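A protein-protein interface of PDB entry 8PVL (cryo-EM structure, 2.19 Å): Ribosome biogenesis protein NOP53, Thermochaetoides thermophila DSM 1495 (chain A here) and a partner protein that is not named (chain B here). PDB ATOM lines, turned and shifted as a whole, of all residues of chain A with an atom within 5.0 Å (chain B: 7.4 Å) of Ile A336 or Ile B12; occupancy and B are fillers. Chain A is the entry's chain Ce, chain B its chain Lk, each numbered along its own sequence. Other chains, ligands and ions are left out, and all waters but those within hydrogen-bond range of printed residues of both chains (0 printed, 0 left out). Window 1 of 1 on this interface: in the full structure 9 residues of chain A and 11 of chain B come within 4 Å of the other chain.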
ATOM      1  N   GLN A 329     -14.804   8.228 -27.483  1.00  0.00           N
ATOM      2  CA  GLN A 329     -13.463   8.508 -27.997  1.00  0.00           C
ATOM      3  C   GLN A 329     -13.024   7.470 -29.027  1.00  0.00           C
ATOM      4  O   GLN A 329     -12.335   7.813 -29.999  1.00  0.00           O
ATOM      5  CB  GLN A 329     -12.461   8.574 -26.849  1.00  0.00           C
ATOM      6  CG  GLN A 329     -12.645   9.766 -25.935  1.00  0.00           C
ATOM      7  CD  GLN A 329     -11.902   9.605 -24.628  1.00  0.00           C
ATOM      8  OE1 GLN A 329     -11.358   8.541 -24.338  1.00  0.00           O
ATOM      9  NE2 GLN A 329     -11.875  10.664 -23.828  1.00  0.00           N
ATOM     10  N   GLN A 332     -14.434   8.554 -32.126  1.00  0.00           N
ATOM     11  CA  GLN A 332     -13.728   9.735 -32.615  1.00  0.00           C
ATOM     12  C   GLN A 332     -12.210   9.552 -32.663  1.00  0.00           C
ATOM     13  O   GLN A 332     -11.473  10.535 -32.515  1.00  0.00           O
ATOM     14  CB  GLN A 332     -14.084  10.949 -31.758  1.00  0.00           C
ATOM     15  CG  GLN A 332     -15.566  11.273 -31.726  1.00  0.00           C
ATOM     16  CD  GLN A 332     -16.087  11.738 -33.070  1.00  0.00           C
ATOM     17  OE1 GLN A 332     -15.393  12.436 -33.809  1.00  0.00           O
ATOM     18  NE2 GLN A 332     -17.316  11.354 -33.394  1.00  0.00           N
ATOM     19  N   ALA A 333     -11.732   8.318 -32.863  1.00  0.00           N
ATOM     20  CA  ALA A 333     -10.299   8.023 -32.792  1.00  0.00           C
ATOM     21  C   ALA A 333      -9.481   8.752 -33.861  1.00  0.00           C
ATOM     22  O   ALA A 333      -8.373   9.223 -33.577  1.00  0.00           O
ATOM     23  CB  ALA A 333     -10.076   6.515 -32.902  1.00  0.00           C
ATOM     24  N   LYS A 334      -9.989   8.830 -35.098  1.00  0.00           N
ATOM     25  CA  LYS A 334      -9.195   9.395 -36.194  1.00  0.00           C
ATOM     26  C   LYS A 334      -8.938  10.888 -36.004  1.00  0.00           C
ATOM     27  O   LYS A 334      -7.826  11.371 -36.262  1.00  0.00           O
ATOM     28  CB  LYS A 334      -9.885   9.139 -37.533  1.00  0.00           C
ATOM     29  CG  LYS A 334      -9.482   7.834 -38.198  1.00  0.00           C
ATOM     30  CD  LYS A 334     -10.642   7.210 -38.956  1.00  0.00           C
ATOM     31  CE  LYS A 334     -10.163   6.504 -40.215  1.00  0.00           C
ATOM     32  NZ  LYS A 334      -8.803   5.924 -40.045  1.00  0.00           N
ATOM     33  N   LYS A 335      -9.954  11.630 -35.554  1.00  0.00           N
ATOM     34  CA  LYS A 335      -9.770  13.046 -35.248  1.00  0.00           C
ATOM     35  C   LYS A 335      -8.778  13.237 -34.109  1.00  0.00           C
ATOM     36  O   LYS A 335      -7.985  14.186 -34.118  1.00  0.00           O
ATOM     37  CB  LYS A 335     -11.113  13.680 -34.893  1.00  0.00           C
ATOM     38  CG  LYS A 335     -11.817  14.363 -36.055  1.00  0.00           C
ATOM     39  CD  LYS A 335     -13.168  14.932 -35.638  1.00  0.00           C
ATOM     40  CE  LYS A 335     -13.095  15.689 -34.316  1.00  0.00           C
ATOM     41  NZ  LYS A 335     -12.164  16.850 -34.381  1.00  0.00           N
ATOM     42  N   ILE A 336      -8.808  12.337 -33.124  1.00  0.00           N
ATOM     43  CA  ILE A 336      -7.870  12.391 -32.005  1.00  0.00           C
ATOM     44  C   ILE A 336      -6.439  12.191 -32.492  1.00  0.00           C
ATOM     45  O   ILE A 336      -5.519  12.907 -32.073  1.00  0.00           O
ATOM     46  CB  ILE A 336      -8.272  11.348 -30.944  1.00  0.00           C
ATOM     47  CG1 ILE A 336      -9.538  11.795 -30.213  1.00  0.00           C
ATOM     48  CG2 ILE A 336      -7.150  11.108 -29.957  1.00  0.00           C
ATOM     49  CD1 ILE A 336     -10.126  10.736 -29.307  1.00  0.00           C
ATOM     50  N   ALA A 337      -6.232  11.230 -33.397  1.00  0.00           N
ATOM     51  CA  ALA A 337      -4.903  11.000 -33.956  1.00  0.00           C
ATOM     52  C   ALA A 337      -4.430  12.195 -34.774  1.00  0.00           C
ATOM     53  O   ALA A 337      -3.247  12.562 -34.726  1.00  0.00           O
ATOM     54  CB  ALA A 337      -4.903   9.733 -34.810  1.00  0.00           C
ATOM     55  N   ALA A 338      -5.345  12.819 -35.526  1.00  0.00           N
ATOM     56  CA  ALA A 338      -4.992  14.024 -36.274  1.00  0.00           C
ATOM     57  C   ALA A 338      -4.588  15.163 -35.341  1.00  0.00           C
ATOM     58  O   ALA A 338      -3.620  15.883 -35.615  1.00  0.00           O
ATOM     59  CB  ALA A 338      -6.160  14.448 -37.164  1.00  0.00           C
ATOM     60  N   GLU A 339      -5.312  15.329 -34.230  1.00  0.00           N
ATOM     61  CA  GLU A 339      -4.966  16.364 -33.257  1.00  0.00           C
ATOM     62  C   GLU A 339      -3.615  16.096 -32.605  1.00  0.00           C
ATOM     63  O   GLU A 339      -2.832  17.028 -32.381  1.00  0.00           O
ATOM     64  CB  GLU A 339      -6.055  16.471 -32.190  1.00  0.00           C
ATOM     65  CG  GLU A 339      -7.372  17.031 -32.690  1.00  0.00           C
ATOM     66  CD  GLU A 339      -8.551  16.564 -31.857  1.00  0.00           C
ATOM     67  OE1 GLU A 339      -8.339  15.764 -30.922  1.00  0.00           O
ATOM     68  OE2 GLU A 339      -9.688  16.997 -32.137  1.00  0.00           O
ATOM     69  N   VAL A 340      -3.330  14.832 -32.281  1.00  0.00           N
ATOM     70  CA  VAL A 340      -2.047  14.483 -31.671  1.00  0.00           C
ATOM     71  C   VAL A 340      -0.900  14.750 -32.642  1.00  0.00           C
ATOM     72  O   VAL A 340       0.140  15.308 -32.261  1.00  0.00           O
ATOM     73  CB  VAL A 340      -2.066  13.019 -31.190  1.00  0.00           C
ATOM     74  CG1 VAL A 340      -0.671  12.547 -30.822  1.00  0.00           C
ATOM     75  CG2 VAL A 340      -2.993  12.869 -29.999  1.00  0.00           C
ATOM     76  N   VAL B   5      -4.478   1.848 -19.613  1.00  0.00           N
ATOM     77  CA  VAL B   5      -4.782   3.153 -20.181  1.00  0.00           C
ATOM     78  C   VAL B   5      -6.271   3.191 -20.483  1.00  0.00           C
ATOM     79  O   VAL B   5      -6.802   2.283 -21.134  1.00  0.00           O
ATOM     80  CB  VAL B   5      -3.952   3.418 -21.447  1.00  0.00           C
ATOM     81  CG1 VAL B   5      -4.113   4.862 -21.894  1.00  0.00           C
ATOM     82  CG2 VAL B   5      -2.494   3.093 -21.194  1.00  0.00           C
ATOM     83  N   ASP B   7      -7.770   6.262 -21.648  1.00  0.00           N
ATOM     84  CA  ASP B   7      -8.003   7.346 -22.590  1.00  0.00           C
ATOM     85  C   ASP B   7      -7.357   7.011 -23.927  1.00  0.00           C
ATOM     86  O   ASP B   7      -6.169   6.663 -23.984  1.00  0.00           O
ATOM     87  CB  ASP B   7      -7.455   8.664 -22.040  1.00  0.00           C
ATOM     88  CG  ASP B   7      -7.888   9.868 -22.853  1.00  0.00           C
ATOM     89  OD1 ASP B   7      -8.813   9.738 -23.678  1.00  0.00           O
ATOM     90  OD2 ASP B   7      -7.296  10.952 -22.664  1.00  0.00           O
ATOM     91  N   ILE B   8      -8.146   7.128 -24.997  1.00  0.00           N
ATOM     92  CA  ILE B   8      -7.670   6.797 -26.337  1.00  0.00           C
ATOM     93  C   ILE B   8      -6.582   7.769 -26.778  1.00  0.00           C
ATOM     94  O   ILE B   8      -5.623   7.378 -27.454  1.00  0.00           O
ATOM     95  CB  ILE B   8      -8.854   6.774 -27.320  1.00  0.00           C
ATOM     96  CG1 ILE B   8      -9.978   5.891 -26.773  1.00  0.00           C
ATOM     97  CG2 ILE B   8      -8.417   6.285 -28.692  1.00  0.00           C
ATOM     98  CD1 ILE B   8      -9.653   4.416 -26.754  1.00  0.00           C
ATOM     99  N   LYS B   9      -6.706   9.042 -26.396  1.00  0.00           N
ATOM    100  CA  LYS B   9      -5.689  10.030 -26.747  1.00  0.00           C
ATOM    101  C   LYS B   9      -4.349   9.707 -26.097  1.00  0.00           C
ATOM    102  O   LYS B   9      -3.305   9.744 -26.761  1.00  0.00           O
ATOM    103  CB  LYS B   9      -6.159  11.428 -26.348  1.00  0.00           C
ATOM    104  CG  LYS B   9      -5.381  12.553 -27.006  1.00  0.00           C
ATOM    105  CD  LYS B   9      -5.353  13.794 -26.136  1.00  0.00           C
ATOM    106  CE  LYS B   9      -4.980  15.023 -26.947  1.00  0.00           C
ATOM    107  NZ  LYS B   9      -5.835  15.168 -28.156  1.00  0.00           N
ATOM    108  N   LYS B  10      -4.364   9.366 -24.805  1.00  0.00           N
ATOM    109  CA  LYS B  10      -3.130   8.984 -24.126  1.00  0.00           C
ATOM    110  C   LYS B  10      -2.560   7.693 -24.694  1.00  0.00           C
ATOM    111  O   LYS B  10      -1.337   7.546 -24.792  1.00  0.00           O
ATOM    112  CB  LYS B  10      -3.368   8.853 -22.623  1.00  0.00           C
ATOM    113  CG  LYS B  10      -4.126  10.015 -22.014  1.00  0.00           C
ATOM    114  CD  LYS B  10      -3.186  11.099 -21.521  1.00  0.00           C
ATOM    115  CE  LYS B  10      -2.957  10.975 -20.024  1.00  0.00           C
ATOM    116  NZ  LYS B  10      -4.199  11.260 -19.253  1.00  0.00           N
ATOM    117  N   PHE B  11      -3.425   6.755 -25.094  1.00  0.00           N
ATOM    118  CA  PHE B  11      -2.930   5.539 -25.733  1.00  0.00           C
ATOM    119  C   PHE B  11      -2.254   5.844 -27.065  1.00  0.00           C
ATOM    120  O   PHE B  11      -1.232   5.234 -27.405  1.00  0.00           O
ATOM    121  CB  PHE B  11      -4.060   4.533 -25.935  1.00  0.00           C
ATOM    122  CG  PHE B  11      -3.579   3.186 -26.374  1.00  0.00           C
ATOM    123  CD1 PHE B  11      -2.981   2.324 -25.469  1.00  0.00           C
ATOM    124  CD2 PHE B  11      -3.689   2.792 -27.696  1.00  0.00           C
ATOM    125  CE1 PHE B  11      -2.524   1.090 -25.869  1.00  0.00           C
ATOM    126  CE2 PHE B  11      -3.234   1.558 -28.101  1.00  0.00           C
ATOM    127  CZ  PHE B  11      -2.644   0.710 -27.187  1.00  0.00           C
ATOM    128  N   ILE B  12      -2.808   6.788 -27.829  1.00  0.00           N
ATOM    129  CA  ILE B  12      -2.209   7.160 -29.108  1.00  0.00           C
ATOM    130  C   ILE B  12      -0.856   7.837 -28.900  1.00  0.00           C
ATOM    131  O   ILE B  12       0.113   7.537 -29.609  1.00  0.00           O
ATOM    132  CB  ILE B  12      -3.188   8.036 -29.915  1.00  0.00           C
ATOM    133  CG1 ILE B  12      -4.333   7.175 -30.451  1.00  0.00           C
ATOM    134  CG2 ILE B  12      -2.488   8.735 -31.068  1.00  0.00           C
ATOM    135  CD1 ILE B  12      -5.386   7.948 -31.207  1.00  0.00           C
ATOM    136  N   GLU B  13      -0.756   8.737 -27.912  1.00  0.00           N
ATOM    137  CA  GLU B  13       0.541   9.354 -27.615  1.00  0.00           C
ATOM    138  C   GLU B  13       1.566   8.325 -27.143  1.00  0.00           C
ATOM    139  O   GLU B  13       2.750   8.409 -27.500  1.00  0.00           O
ATOM    140  CB  GLU B  13       0.398  10.466 -26.574  1.00  0.00           C
ATOM    141  CG  GLU B  13      -0.678  11.488 -26.857  1.00  0.00           C
ATOM    142  CD  GLU B  13      -1.238  12.100 -25.588  1.00  0.00           C
ATOM    143  OE1 GLU B  13      -0.683  11.830 -24.502  1.00  0.00           O
ATOM    144  OE2 GLU B  13      -2.230  12.850 -25.674  1.00  0.00           O
ATOM    145  N   ILE B  14       1.128   7.348 -26.342  1.00  0.00           N
ATOM    146  CA  ILE B  14       2.023   6.276 -25.906  1.00  0.00           C
ATOM    147  C   ILE B  14       2.508   5.465 -27.102  1.00  0.00           C
ATOM    148  O   ILE B  14       3.695   5.129 -27.203  1.00  0.00           O
ATOM    149  CB  ILE B  14       1.317   5.394 -24.856  1.00  0.00           C
ATOM    150  CG1 ILE B  14       1.276   6.105 -23.505  1.00  0.00           C
ATOM    151  CG2 ILE B  14       2.010   4.053 -24.703  1.00  0.00           C
ATOM    152  CD1 ILE B  14       0.372   5.436 -22.497  1.00  0.00           C
ATOM    153  N   CYS B  15       1.606   5.162 -28.039  1.00  0.00           N
ATOM    154  CA  CYS B  15       1.998   4.418 -29.233  1.00  0.00           C
ATOM    155  C   CYS B  15       2.920   5.228 -30.137  1.00  0.00           C
ATOM    156  O   CYS B  15       3.724   4.648 -30.875  1.00  0.00           O
ATOM    157  CB  CYS B  15       0.757   3.971 -30.003  1.00  0.00           C
ATOM    158  SG  CYS B  15      -0.033   2.505 -29.314  1.00  0.00           S
ATOM    159  N   ARG B  16       2.824   6.555 -30.098  1.00  0.00           N
ATOM    160  CA  ARG B  16       3.744   7.400 -30.852  1.00  0.00           C
ATOM    161  C   ARG B  16       5.004   7.771 -30.075  1.00  0.00           C
ATOM    162  O   ARG B  16       5.839   8.508 -30.608  1.00  0.00           O
ATOM    163  CB  ARG B  16       3.045   8.678 -31.325  1.00  0.00           C
ATOM    164  CG  ARG B  16       1.815   8.429 -32.169  1.00  0.00           C
ATOM    165  CD  ARG B  16       1.071   9.718 -32.468  1.00  0.00           C
ATOM    166  NE  ARG B  16       1.899  10.689 -33.173  1.00  0.00           N
ATOM    167  CZ  ARG B  16       2.229  10.615 -34.455  1.00  0.00           C
ATOM    168  NH1 ARG B  16       1.791   9.636 -35.230  1.00  0.00           N
ATOM    169  NH2 ARG B  16       3.013  11.554 -34.978  1.00  0.00           N
ATOM    170  N   ARG B  17       5.155   7.301 -28.837  1.00  0.00           N
ATOM    171  CA  ARG B  17       6.410   7.500 -28.119  1.00  0.00           C
ATOM    172  C   ARG B  17       7.557   6.758 -28.804  1.00  0.00           C
ATOM    173  O   ARG B  17       7.367   5.716 -29.436  1.00  0.00           O
ATOM    174  CB  ARG B  17       6.284   7.032 -26.668  1.00  0.00           C
ATOM    175  CG  ARG B  17       5.723   8.078 -25.723  1.00  0.00           C
ATOM    176  CD  ARG B  17       5.290   7.465 -24.402  1.00  0.00           C
ATOM    177  NE  ARG B  17       6.303   6.580 -23.841  1.00  0.00           N
ATOM    178  CZ  ARG B  17       6.243   6.050 -22.626  1.00  0.00           C
ATOM    179  NH1 ARG B  17       5.228   6.300 -21.816  1.00  0.00           N
ATOM    180  NH2 ARG B  17       7.223   5.251 -22.217  1.00  0.00           N
ATOM    181  N   LEU B  60      -4.783  -1.242 -23.245  1.00  0.00           N
ATOM    182  CA  LEU B  60      -6.071  -0.592 -23.439  1.00  0.00           C
ATOM    183  C   LEU B  60      -7.119  -1.661 -23.708  1.00  0.00           C
ATOM    184  O   LEU B  60      -6.936  -2.507 -24.589  1.00  0.00           O
ATOM    185  CB  LEU B  60      -6.011   0.406 -24.597  1.00  0.00           C
ATOM    186  CG  LEU B  60      -7.337   0.933 -25.146  1.00  0.00           C
ATOM    187  CD1 LEU B  60      -7.978   1.920 -24.188  1.00  0.00           C
ATOM    188  CD2 LEU B  60      -7.123   1.568 -26.504  1.00  0.00           C
ATOM    189  N   LEU B  71      -9.137   1.163 -34.950  1.00  0.00           N
ATOM    190  CA  LEU B  71      -8.113   1.813 -34.127  1.00  0.00           C
ATOM    191  C   LEU B  71      -6.702   1.437 -34.582  1.00  0.00           C
ATOM    192  O   LEU B  71      -5.766   2.241 -34.453  1.00  0.00           O
ATOM    193  CB  LEU B  71      -8.315   1.447 -32.655  1.00  0.00           C
ATOM    194  CG  LEU B  71      -7.377   2.099 -31.635  1.00  0.00           C
ATOM    195  CD1 LEU B  71      -7.556   3.609 -31.629  1.00  0.00           C
ATOM    196  CD2 LEU B  71      -7.595   1.526 -30.248  1.00  0.00           C
ATOM    197  N   SER B  74      -5.527   3.949 -37.087  1.00  0.00           N
ATOM    198  CA  SER B  74      -5.051   5.185 -36.476  1.00  0.00           C
ATOM    199  C   SER B  74      -3.742   4.993 -35.723  1.00  0.00           C
ATOM    200  O   SER B  74      -3.060   5.981 -35.430  1.00  0.00           O
ATOM    201  CB  SER B  74      -6.110   5.750 -35.528  1.00  0.00           C
ATOM    202  OG  SER B  74      -7.383   5.776 -36.148  1.00  0.00           O
ATOM    203  N   LEU B  75      -3.397   3.752 -35.391  1.00  0.00           N
ATOM    204  CA  LEU B  75      -2.100   3.468 -34.795  1.00  0.00           C
ATOM    205  C   LEU B  75      -0.976   3.774 -35.791  1.00  0.00           C
ATOM    206  O   LEU B  75      -1.191   3.733 -37.005  1.00  0.00           O
ATOM    207  CB  LEU B  75      -2.034   2.005 -34.355  1.00  0.00           C
ATOM    208  CG  LEU B  75      -2.649   1.647 -32.998  1.00  0.00           C
ATOM    209  CD1 LEU B  75      -1.982   0.408 -32.425  1.00  0.00           C
ATOM    210  CD2 LEU B  75      -2.569   2.804 -32.011  1.00  0.00           C
ATOM    211  N   PRO B  76       0.219   4.121 -35.303  1.00  0.00           N
ATOM    212  CA  PRO B  76       1.335   4.471 -36.207  1.00  0.00           C
ATOM    213  C   PRO B  76       1.749   3.300 -37.079  1.00  0.00           C
ATOM    214  O   PRO B  76       1.711   2.140 -36.642  1.00  0.00           O
ATOM    215  CB  PRO B  76       2.464   4.863 -35.241  1.00  0.00           C
ATOM    216  CG  PRO B  76       1.777   5.259 -34.001  1.00  0.00           C
ATOM    217  CD  PRO B  76       0.565   4.390 -33.895  1.00  0.00           C
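The side-chain carboxylate of Glu A339 is in salt-bridge range of the side-chain amino group of Lys A335 (3.3 Å).
Printed residues of chain A that touch a printed residue of chain B: Gln A329, Lys A334, Ile A336, Glu A339 and Val A340.
Hydrophobic or aromatic side chains of chain A that line the printed part of chain B: Ile A336 and Val A340.
Of the 17 printed residues of chain B, 6 touch a printed residue of chain A.
Among the printed residues, 8 pairs touch across the chains.
Among the printed residues, Asp or Glu carboxylates within 4 Å of a Lys or Arg side-chain nitrogen of the other chain: Glu A339 with Lys B9.
The side-chain carboxylate of Glu A339 is in salt-bridge range of the side-chain amino group of Lys B9 (3.8 Å).
The side-chain amide oxygen of Gln A329 lies close to the side-chain carboxylate of Asp B7 (2.9 Å).
Ile A336 touches just these residues of chain B: Lys B9 and Ile B12.
Ile B12 touches one residue of chain A.
Printed residues of chain B within 4 Å of Glu A339: Lys B9.
Printed residues of chain B within 4 Å of Lys A334: Ser B74 (3.6 Å).
Of the printed residues of chain A, Asp B7 touches Gln A329 (2.9 Å).
Ala A338 touches none of the printed residues of chain B.
The nearest residue of chain B that does not touch Ile A336 is Ile B8 (4.6 Å).
The nearest printed residue of chain A that does not touch Ile B12 is Ala A333 (4.02 Å).
Gln A329 touches Ile B8 (OE1 to N, 3.6 Å).
Lys A334 touches Ser B74.
Lys B9 touches Ile A336 (CA to CG2, 3.7 Å).
CG2 of Ile A336 touches CD1 of Ile B12, at 3.8 Å.
Lys B9 touches Val A340.
CG1 of Val A340 touches CD of Arg B16, at 3.7 Å.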
